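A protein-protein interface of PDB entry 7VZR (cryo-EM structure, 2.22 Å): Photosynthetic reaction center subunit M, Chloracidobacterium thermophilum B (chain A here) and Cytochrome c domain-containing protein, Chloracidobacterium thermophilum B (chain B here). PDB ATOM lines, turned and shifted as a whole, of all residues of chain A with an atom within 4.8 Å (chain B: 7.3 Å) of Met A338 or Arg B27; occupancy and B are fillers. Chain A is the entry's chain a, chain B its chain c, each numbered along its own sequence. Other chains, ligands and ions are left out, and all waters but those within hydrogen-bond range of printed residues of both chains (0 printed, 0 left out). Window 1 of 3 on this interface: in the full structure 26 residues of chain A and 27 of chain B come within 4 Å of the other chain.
Met A334 touches none of the printed residues of chain B.
Of chain B, only Arg B27 (3.6 Å) comes within 4 Å of Met A338.
Of the printed residues of chain A, Ile B23 touches Thr A51 (3.0 Å).
Printed residues of chain A within 4 Å of Tyr B133: Asn A339 (3.9 Å).
NH1 of Arg A63 lies close to SD of Met A338 (3.8 Å).
OE1 of Gln B129 sits at hydrogen-bond distance from NH1 of Arg B11 (3.5 Å).
The backbone carbonyl oxygen (O) of Ile B23 is in hydrogen-bond range of the side-chain hydroxyl (OG) of Ser B26, at 3.2 Å.
The side-chain carboxylate of Asp A55 lies within salt-bridge range of the guanidinium group of Arg A63, 3.1 Å away.
NH1 of Arg B11 is in hydrogen-bond range of O of Ser B26 (3.3 Å).
Thr A51 touches Ile B23.
Arg B11 touches Trp A53.
CA of Arg B11 touches OD1 of Asn A54, 3.2 Å away.
C of Asn A54 touches NH2 of Arg B27 (3.9 Å).
NH2 of Arg A63 touches NH2 of Arg B27, at 3.8 Å.
O of Pro A74 touches CB of Thr B28, at 3.5 Å.
Ala B29 touches Asp A337 (CB to O, 3.7 Å).
CB of Arg B27 touches O of Met A338 (3.6 Å).
Tyr B32 touches Asn A339.
Asn A339 touches Tyr B133 (OD1 to CE1, 3.9 Å).
NH1 of Arg B27 sits at hydrogen-bond distance from O of Thr A51 (3.1 Å).
O of Trp A53 sits at hydrogen-bond distance from NH2 of Arg B27, at 3.2 Å.
The side-chain hydroxyl (OH) of Tyr B32 is in hydrogen-bond range of the backbone carbonyl oxygen (O) of Asp A337 (2.9 Å).
The backbone carbonyl oxygen (O) of Asn A339 is in hydrogen-bond range of the guanidinium group (NH2) of Arg B11 (3.1 Å).
OD2 of Asp A55 lies within salt-bridge range of NH2 of Arg B11 (3.3 Å).
The side-chain amide nitrogen (NE2) of Gln B129 sits at hydrogen-bond distance from the side-chain amide oxygen (OD1) of Asn A339 (3.5 Å).
NE of Arg B27 lies within salt-bridge range of OD1 of Asp A55, at 3.5 Å.
OD1 of Asn A339 sits close to O of Ser B26 (3.2 Å).
Of the 15 printed residues of chain B, 9 touch a printed residue of chain A.
Along chain B the printed residues that touch a printed residue of chain A span positions 11 to 133.
Of the 15 printed residues of chain A, 9 touch a printed residue of chain B.
Hydrophobic or aromatic side chains of chain A within 4 Å of the printed part of chain B: Met A338.
Among the printed residues, 18 pairs touch across the chains.
Among the printed residues, Asp or Glu carboxylates within 4 Å of a Lys or Arg side-chain nitrogen of the other chain: Asp A55 with Arg B11 and Asp A55 with Arg B27.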
ATOM      1  N   THR A  51      21.802  12.024   8.214  1.00  0.00           N
ATOM      2  CA  THR A  51      20.991  10.935   7.702  1.00  0.00           C
ATOM      3  C   THR A  51      19.619  10.854   8.344  1.00  0.00           C
ATOM      4  O   THR A  51      18.771  10.167   7.833  1.00  0.00           O
ATOM      5  CB  THR A  51      21.746   9.628   7.791  1.00  0.00           C
ATOM      6  OG1 THR A  51      22.529   9.569   8.967  1.00  0.00           O
ATOM      7  CG2 THR A  51      22.643   9.572   6.752  1.00  0.00           C
ATOM      8  N   TRP A  53      17.535  13.334   8.098  1.00  0.00           N
ATOM      9  CA  TRP A  53      16.633  14.251   7.425  1.00  0.00           C
ATOM     10  C   TRP A  53      16.049  13.640   6.146  1.00  0.00           C
ATOM     11  O   TRP A  53      16.605  12.763   5.552  1.00  0.00           O
ATOM     12  CB  TRP A  53      17.321  15.604   7.178  1.00  0.00           C
ATOM     13  CG  TRP A  53      18.004  16.240   8.370  1.00  0.00           C
ATOM     14  CD1 TRP A  53      19.266  16.566   8.446  1.00  0.00           C
ATOM     15  CD2 TRP A  53      17.446  16.516   9.644  1.00  0.00           C
ATOM     16  NE1 TRP A  53      19.560  17.074   9.630  1.00  0.00           N
ATOM     17  CE2 TRP A  53      18.453  17.072  10.409  1.00  0.00           C
ATOM     18  CE3 TRP A  53      16.174  16.391  10.201  1.00  0.00           C
ATOM     19  CZ2 TRP A  53      18.258  17.452  11.731  1.00  0.00           C
ATOM     20  CZ3 TRP A  53      15.974  16.794  11.491  1.00  0.00           C
ATOM     21  CH2 TRP A  53      17.021  17.277  12.252  1.00  0.00           C
ATOM     22  N   ASN A  54      14.841  14.032   5.822  1.00  0.00           N
ATOM     23  CA  ASN A  54      14.274  13.835   4.503  1.00  0.00           C
ATOM     24  C   ASN A  54      15.239  14.257   3.380  1.00  0.00           C
ATOM     25  O   ASN A  54      16.089  15.112   3.522  1.00  0.00           O
ATOM     26  CB  ASN A  54      12.925  14.566   4.383  1.00  0.00           C
ATOM     27  CG  ASN A  54      11.758  13.773   4.918  1.00  0.00           C
ATOM     28  OD1 ASN A  54      11.777  12.610   4.915  1.00  0.00           O
ATOM     29  ND2 ASN A  54      10.740  14.407   5.269  1.00  0.00           N
ATOM     30  N   ASP A  55      15.064  13.635   2.242  1.00  0.00           N
ATOM     31  CA  ASP A  55      15.650  14.160   1.026  1.00  0.00           C
ATOM     32  C   ASP A  55      15.001  15.473   0.656  1.00  0.00           C
ATOM     33  O   ASP A  55      13.808  15.651   0.817  1.00  0.00           O
ATOM     34  CB  ASP A  55      15.504  13.187  -0.118  1.00  0.00           C
ATOM     35  CG  ASP A  55      16.098  11.847   0.147  1.00  0.00           C
ATOM     36  OD1 ASP A  55      16.934  11.690   0.993  1.00  0.00           O
ATOM     37  OD2 ASP A  55      15.725  10.904  -0.492  1.00  0.00           O
ATOM     38  N   ARG A  63      24.984  15.477  -2.075  1.00  0.00           N
ATOM     39  CA  ARG A  63      25.344  14.088  -1.813  1.00  0.00           C
ATOM     40  C   ARG A  63      26.267  13.343  -2.820  1.00  0.00           C
ATOM     41  O   ARG A  63      27.151  12.662  -2.355  1.00  0.00           O
ATOM     42  CB  ARG A  63      24.041  13.301  -1.537  1.00  0.00           C
ATOM     43  CG  ARG A  63      24.306  11.974  -0.887  1.00  0.00           C
ATOM     44  CD  ARG A  63      23.112  11.136  -0.594  1.00  0.00           C
ATOM     45  NE  ARG A  63      22.081  11.784   0.178  1.00  0.00           N
ATOM     46  CZ  ARG A  63      20.802  11.437   0.259  1.00  0.00           C
ATOM     47  NH1 ARG A  63      20.300  10.414  -0.379  1.00  0.00           N
ATOM     48  NH2 ARG A  63      20.007  12.204   0.962  1.00  0.00           N
ATOM     49  N   ILE A  67      29.641  11.656  -1.307  1.00  0.00           N
ATOM     50  CA  ILE A  67      29.970  10.250  -1.536  1.00  0.00           C
ATOM     51  C   ILE A  67      31.343  10.097  -2.173  1.00  0.00           C
ATOM     52  O   ILE A  67      32.199   9.443  -1.622  1.00  0.00           O
ATOM     53  CB  ILE A  67      28.898   9.546  -2.383  1.00  0.00           C
ATOM     54  CG1 ILE A  67      27.532   9.522  -1.733  1.00  0.00           C
ATOM     55  CG2 ILE A  67      29.326   8.215  -2.703  1.00  0.00           C
ATOM     56  CD1 ILE A  67      26.438   9.188  -2.667  1.00  0.00           C
ATOM     57  N   TYR A  72      30.345  10.968   3.103  1.00  0.00           N
ATOM     58  CA  TYR A  72      29.080  10.288   3.169  1.00  0.00           C
ATOM     59  C   TYR A  72      29.239   8.857   2.732  1.00  0.00           C
ATOM     60  O   TYR A  72      29.408   8.609   1.544  1.00  0.00           O
ATOM     61  CB  TYR A  72      28.088  10.983   2.272  1.00  0.00           C
ATOM     62  CG  TYR A  72      26.705  10.587   2.481  1.00  0.00           C
ATOM     63  CD1 TYR A  72      26.246   9.345   2.090  1.00  0.00           C
ATOM     64  CD2 TYR A  72      25.819  11.451   3.071  1.00  0.00           C
ATOM     65  CE1 TYR A  72      25.021   8.997   2.309  1.00  0.00           C
ATOM     66  CE2 TYR A  72      24.584  11.114   3.228  1.00  0.00           C
ATOM     67  CZ  TYR A  72      24.189   9.896   2.874  1.00  0.00           C
ATOM     68  OH  TYR A  72      22.923   9.606   3.079  1.00  0.00           O
ATOM     69  N   PRO A  74      27.739   5.427   1.788  1.00  0.00           N
ATOM     70  CA  PRO A  74      26.449   4.873   1.396  1.00  0.00           C
ATOM     71  C   PRO A  74      26.004   3.612   2.131  1.00  0.00           C
ATOM     72  O   PRO A  74      24.817   3.343   2.143  1.00  0.00           O
ATOM     73  CB  PRO A  74      26.670   4.598  -0.083  1.00  0.00           C
ATOM     74  CG  PRO A  74      27.852   5.291  -0.435  1.00  0.00           C
ATOM     75  CD  PRO A  74      28.703   5.255   0.718  1.00  0.00           C
ATOM     76  N   MET A 334      24.654   6.165  -8.186  1.00  0.00           N
ATOM     77  CA  MET A 334      24.476   5.731  -6.822  1.00  0.00           C
ATOM     78  C   MET A 334      23.279   6.372  -6.158  1.00  0.00           C
ATOM     79  O   MET A 334      22.678   5.745  -5.309  1.00  0.00           O
ATOM     80  CB  MET A 334      25.710   5.998  -5.995  1.00  0.00           C
ATOM     81  CG  MET A 334      25.879   5.087  -4.856  1.00  0.00           C
ATOM     82  SD  MET A 334      27.606   4.862  -4.462  1.00  0.00           S
ATOM     83  CE  MET A 334      27.678   3.202  -3.957  1.00  0.00           C
ATOM     84  N   LEU A 335      22.928   7.617  -6.492  1.00  0.00           N
ATOM     85  CA  LEU A 335      21.636   8.109  -5.975  1.00  0.00           C
ATOM     86  C   LEU A 335      20.455   7.270  -6.456  1.00  0.00           C
ATOM     87  O   LEU A 335      19.514   7.012  -5.716  1.00  0.00           O
ATOM     88  CB  LEU A 335      21.386   9.567  -6.330  1.00  0.00           C
ATOM     89  CG  LEU A 335      21.652  10.685  -5.356  1.00  0.00           C
ATOM     90  CD1 LEU A 335      22.987  10.547  -4.663  1.00  0.00           C
ATOM     91  CD2 LEU A 335      21.518  11.942  -6.062  1.00  0.00           C
ATOM     92  N   ASN A 336      20.499   6.804  -7.687  1.00  0.00           N
ATOM     93  CA  ASN A 336      19.362   5.941  -8.054  1.00  0.00           C
ATOM     94  C   ASN A 336      19.195   4.686  -7.183  1.00  0.00           C
ATOM     95  O   ASN A 336      18.105   4.164  -7.106  1.00  0.00           O
ATOM     96  CB  ASN A 336      19.397   5.527  -9.498  1.00  0.00           C
ATOM     97  CG  ASN A 336      19.363   6.678 -10.391  1.00  0.00           C
ATOM     98  OD1 ASN A 336      19.060   7.706  -9.960  1.00  0.00           O
ATOM     99  ND2 ASN A 336      19.833   6.545 -11.543  1.00  0.00           N
ATOM    100  N   ASP A 337      20.057   4.234  -6.323  1.00  0.00           N
ATOM    101  CA  ASP A 337      19.729   3.118  -5.415  1.00  0.00           C
ATOM    102  C   ASP A 337      19.472   3.522  -3.991  1.00  0.00           C
ATOM    103  O   ASP A 337      19.539   2.701  -3.175  1.00  0.00           O
ATOM    104  CB  ASP A 337      20.766   1.996  -5.345  1.00  0.00           C
ATOM    105  CG  ASP A 337      21.194   1.521  -6.604  1.00  0.00           C
ATOM    106  OD1 ASP A 337      20.473   1.448  -7.560  1.00  0.00           O
ATOM    107  OD2 ASP A 337      22.302   1.138  -6.668  1.00  0.00           O
ATOM    108  N   MET A 338      19.260   4.759  -3.646  1.00  0.00           N
ATOM    109  CA  MET A 338      19.163   5.146  -2.276  1.00  0.00           C
ATOM    110  C   MET A 338      17.764   5.409  -1.759  1.00  0.00           C
ATOM    111  O   MET A 338      17.658   6.031  -0.835  1.00  0.00           O
ATOM    112  CB  MET A 338      20.022   6.365  -2.028  1.00  0.00           C
ATOM    113  CG  MET A 338      21.504   6.257  -2.221  1.00  0.00           C
ATOM    114  SD  MET A 338      22.515   7.628  -1.611  1.00  0.00           S
ATOM    115  CE  MET A 338      22.861   6.983  -0.032  1.00  0.00           C
ATOM    116  N   ASN A 339      16.765   4.823  -2.348  1.00  0.00           N
ATOM    117  CA  ASN A 339      15.380   4.979  -2.100  1.00  0.00           C
ATOM    118  C   ASN A 339      15.067   6.498  -1.875  1.00  0.00           C
ATOM    119  O   ASN A 339      14.665   6.881  -0.896  1.00  0.00           O
ATOM    120  CB  ASN A 339      14.918   3.846  -1.055  1.00  0.00           C
ATOM    121  CG  ASN A 339      13.556   3.979  -0.513  1.00  0.00           C
ATOM    122  OD1 ASN A 339      13.371   4.017   0.613  1.00  0.00           O
ATOM    123  ND2 ASN A 339      12.650   4.026  -1.289  1.00  0.00           N
ATOM    124  N   VAL A 340      15.225   7.318  -2.876  1.00  0.00           N
ATOM    125  CA  VAL A 340      15.071   8.768  -2.771  1.00  0.00           C
ATOM    126  C   VAL A 340      13.604   9.180  -2.727  1.00  0.00           C
ATOM    127  O   VAL A 340      12.797   8.783  -3.563  1.00  0.00           O
ATOM    128  CB  VAL A 340      15.856   9.467  -3.890  1.00  0.00           C
ATOM    129  CG1 VAL A 340      15.430  10.868  -4.135  1.00  0.00           C
ATOM    130  CG2 VAL A 340      17.292   9.432  -3.642  1.00  0.00           C
ATOM    131  N   ARG B  11      13.166  11.941   8.176  1.00  0.00           N
ATOM    132  CA  ARG B  11      12.718  10.871   7.378  1.00  0.00           C
ATOM    133  C   ARG B  11      11.889   9.762   8.042  1.00  0.00           C
ATOM    134  O   ARG B  11      12.197   9.356   9.001  1.00  0.00           O
ATOM    135  CB  ARG B  11      13.971  10.170   6.808  1.00  0.00           C
ATOM    136  CG  ARG B  11      13.704   9.469   5.538  1.00  0.00           C
ATOM    137  CD  ARG B  11      14.509   8.345   5.050  1.00  0.00           C
ATOM    138  NE  ARG B  11      14.440   8.698   3.702  1.00  0.00           N
ATOM    139  CZ  ARG B  11      14.405   7.995   2.597  1.00  0.00           C
ATOM    140  NH1 ARG B  11      14.382   6.787   2.512  1.00  0.00           N
ATOM    141  NH2 ARG B  11      14.319   8.675   1.567  1.00  0.00           N
ATOM    142  N   SER B  22      17.611   2.922  11.899  1.00  0.00           N
ATOM    143  CA  SER B  22      16.608   2.551  10.979  1.00  0.00           C
ATOM    144  C   SER B  22      16.442   3.534   9.867  1.00  0.00           C
ATOM    145  O   SER B  22      16.116   3.151   8.840  1.00  0.00           O
ATOM    146  CB  SER B  22      15.302   2.274  11.640  1.00  0.00           C
ATOM    147  OG  SER B  22      14.871   3.439  12.244  1.00  0.00           O
ATOM    148  N   ILE B  23      16.759   4.777  10.110  1.00  0.00           N
ATOM    149  CA  ILE B  23      16.678   5.784   9.127  1.00  0.00           C
ATOM    150  C   ILE B  23      17.739   5.560   8.163  1.00  0.00           C
ATOM    151  O   ILE B  23      17.523   5.643   7.042  1.00  0.00           O
ATOM    152  CB  ILE B  23      16.695   7.213   9.684  1.00  0.00           C
ATOM    153  CG1 ILE B  23      15.456   7.430  10.486  1.00  0.00           C
ATOM    154  CG2 ILE B  23      16.585   8.208   8.557  1.00  0.00           C
ATOM    155  CD1 ILE B  23      15.448   8.661  11.284  1.00  0.00           C
ATOM    156  N   ALA B  24      18.899   5.231   8.612  1.00  0.00           N
ATOM    157  CA  ALA B  24      19.974   4.955   7.728  1.00  0.00           C
ATOM    158  C   ALA B  24      19.666   3.789   6.930  1.00  0.00           C
ATOM    159  O   ALA B  24      19.757   3.897   5.793  1.00  0.00           O
ATOM    160  CB  ALA B  24      21.284   4.792   8.413  1.00  0.00           C
ATOM    161  N   ALA B  25      19.164   2.714   7.516  1.00  0.00           N
ATOM    162  CA  ALA B  25      18.771   1.511   6.842  1.00  0.00           C
ATOM    163  C   ALA B  25      17.836   1.704   5.731  1.00  0.00           C
ATOM    164  O   ALA B  25      17.987   1.148   4.750  1.00  0.00           O
ATOM    165  CB  ALA B  25      18.209   0.530   7.781  1.00  0.00           C
ATOM    166  N   SER B  26      16.986   2.668   5.818  1.00  0.00           N
ATOM    167  CA  SER B  26      16.079   2.936   4.773  1.00  0.00           C
ATOM    168  C   SER B  26      16.566   3.618   3.533  1.00  0.00           C
ATOM    169  O   SER B  26      15.810   3.842   2.747  1.00  0.00           O
ATOM    170  CB  SER B  26      14.867   3.543   5.273  1.00  0.00           C
ATOM    171  OG  SER B  26      14.978   4.854   5.221  1.00  0.00           O
ATOM    172  N   ARG B  27      17.834   3.928   3.423  1.00  0.00           N
ATOM    173  CA  ARG B  27      18.441   4.412   2.255  1.00  0.00           C
ATOM    174  C   ARG B  27      19.544   3.515   1.874  1.00  0.00           C
ATOM    175  O   ARG B  27      20.105   3.753   0.974  1.00  0.00           O
ATOM    176  CB  ARG B  27      19.063   5.755   2.418  1.00  0.00           C
ATOM    177  CG  ARG B  27      18.379   6.767   3.192  1.00  0.00           C
ATOM    178  CD  ARG B  27      19.206   7.985   3.178  1.00  0.00           C
ATOM    179  NE  ARG B  27      18.399   9.067   2.765  1.00  0.00           N
ATOM    180  CZ  ARG B  27      17.954  10.016   3.553  1.00  0.00           C
ATOM    181  NH1 ARG B  27      18.196  10.030   4.830  1.00  0.00           N
ATOM    182  NH2 ARG B  27      17.182  10.883   3.059  1.00  0.00           N
ATOM    183  N   THR B  28      19.870   2.493   2.603  1.00  0.00           N
ATOM    184  CA  THR B  28      20.973   1.616   2.200  1.00  0.00           C
ATOM    185  C   THR B  28      20.482   0.363   1.615  1.00  0.00           C
ATOM    186  O   THR B  28      20.080  -0.397   2.299  1.00  0.00           O
ATOM    187  CB  THR B  28      22.095   1.501   3.265  1.00  0.00           C
ATOM    188  OG1 THR B  28      22.918   0.434   3.023  1.00  0.00           O
ATOM    189  CG2 THR B  28      21.667   1.144   4.333  1.00  0.00           C
ATOM    190  N   ALA B  29      20.430   0.270   0.320  1.00  0.00           N
ATOM    191  CA  ALA B  29      19.935  -0.868  -0.454  1.00  0.00           C
ATOM    192  C   ALA B  29      20.136  -2.259   0.106  1.00  0.00           C
ATOM    193  O   ALA B  29      19.221  -2.866   0.385  1.00  0.00           O
ATOM    194  CB  ALA B  29      20.221  -0.760  -1.925  1.00  0.00           C
ATOM    195  N   PRO B  30      21.354  -2.695   0.380  1.00  0.00           N
ATOM    196  CA  PRO B  30      21.487  -3.955   1.107  1.00  0.00           C
ATOM    197  C   PRO B  30      20.746  -4.023   2.473  1.00  0.00           C
ATOM    198  O   PRO B  30      20.539  -5.086   2.800  1.00  0.00           O
ATOM    199  CB  PRO B  30      22.942  -4.119   1.301  1.00  0.00           C
ATOM    200  CG  PRO B  30      23.505  -2.843   1.059  1.00  0.00           C
ATOM    201  CD  PRO B  30      22.615  -2.008   0.301  1.00  0.00           C
ATOM    202  N   ALA B  31      20.391  -3.021   3.220  1.00  0.00           N
ATOM    203  CA  ALA B  31      19.626  -3.205   4.412  1.00  0.00           C
ATOM    204  C   ALA B  31      18.184  -3.243   4.053  1.00  0.00           C
ATOM    205  O   ALA B  31      17.552  -4.010   4.514  1.00  0.00           O
ATOM    206  CB  ALA B  31      19.879  -2.080   5.406  1.00  0.00           C
ATOM    207  N   TYR B  32      17.656  -2.312   3.308  1.00  0.00           N
ATOM    208  CA  TYR B  32      16.292  -2.335   2.922  1.00  0.00           C
ATOM    209  C   TYR B  32      15.882  -3.572   2.129  1.00  0.00           C
ATOM    210  O   TYR B  32      14.783  -3.960   2.280  1.00  0.00           O
ATOM    211  CB  TYR B  32      15.770  -0.998   2.401  1.00  0.00           C
ATOM    212  CG  TYR B  32      16.182  -0.483   1.073  1.00  0.00           C
ATOM    213  CD1 TYR B  32      15.752  -1.084  -0.100  1.00  0.00           C
ATOM    214  CD2 TYR B  32      16.956   0.669   0.984  1.00  0.00           C
ATOM    215  CE1 TYR B  32      16.093  -0.550  -1.332  1.00  0.00           C
ATOM    216  CE2 TYR B  32      17.214   1.222  -0.217  1.00  0.00           C
ATOM    217  CZ  TYR B  32      16.849   0.572  -1.353  1.00  0.00           C
ATOM    218  OH  TYR B  32      17.181   1.120  -2.495  1.00  0.00           O
ATOM    219  N   GLN B 129       6.554   3.043   3.817  1.00  0.00           N
ATOM    220  CA  GLN B 129       7.929   2.814   3.660  1.00  0.00           C
ATOM    221  C   GLN B 129       8.304   1.317   3.418  1.00  0.00           C
ATOM    222  O   GLN B 129       9.163   1.131   2.692  1.00  0.00           O
ATOM    223  CB  GLN B 129       8.699   3.514   4.752  1.00  0.00           C
ATOM    224  CG  GLN B 129      10.164   3.528   4.527  1.00  0.00           C
ATOM    225  CD  GLN B 129      10.702   4.508   3.497  1.00  0.00           C
ATOM    226  OE1 GLN B 129      11.504   5.354   3.817  1.00  0.00           O
ATOM    227  NE2 GLN B 129      10.340   4.327   2.277  1.00  0.00           N
ATOM    228  N   TYR B 133      10.193  -0.440  -0.067  1.00  0.00           N
ATOM    229  CA  TYR B 133      11.196  -1.494  -0.050  1.00  0.00           C
ATOM    230  C   TYR B 133      10.821  -2.674  -0.936  1.00  0.00           C
ATOM    231  O   TYR B 133      11.689  -3.212  -1.618  1.00  0.00           O
ATOM    232  CB  TYR B 133      11.520  -2.048   1.339  1.00  0.00           C
ATOM    233  CG  TYR B 133      11.916  -1.095   2.374  1.00  0.00           C
ATOM    234  CD1 TYR B 133      12.300   0.190   2.067  1.00  0.00           C
ATOM    235  CD2 TYR B 133      11.891  -1.468   3.677  1.00  0.00           C
ATOM    236  CE1 TYR B 133      12.652   1.043   2.973  1.00  0.00           C
ATOM    237  CE2 TYR B 133      12.176  -0.594   4.612  1.00  0.00           C
ATOM    238  CZ  TYR B 133      12.566   0.672   4.248  1.00  0.00           C
ATOM    239  OH  TYR B 133      12.933   1.538   5.188  1.00  0.00           O
ATOM    240  N   GLU B 136      11.264  -2.006  -4.692  1.00  0.00           N
ATOM    241  CA  GLU B 136      12.682  -2.150  -4.981  1.00  0.00           C
ATOM    242  C   GLU B 136      13.141  -3.620  -5.129  1.00  0.00           C
ATOM    243  O   GLU B 136      13.749  -3.985  -6.130  1.00  0.00           O
ATOM    244  CB  GLU B 136      13.498  -1.425  -3.900  1.00  0.00           C
ATOM    245  CG  GLU B 136      13.478   0.002  -3.895  1.00  0.00           C
ATOM    246  CD  GLU B 136      13.668   0.616  -5.190  1.00  0.00           C
ATOM    247  OE1 GLU B 136      12.973   1.562  -5.511  1.00  0.00           O
ATOM    248  OE2 GLU B 136      14.525   0.209  -5.940  1.00  0.00           O
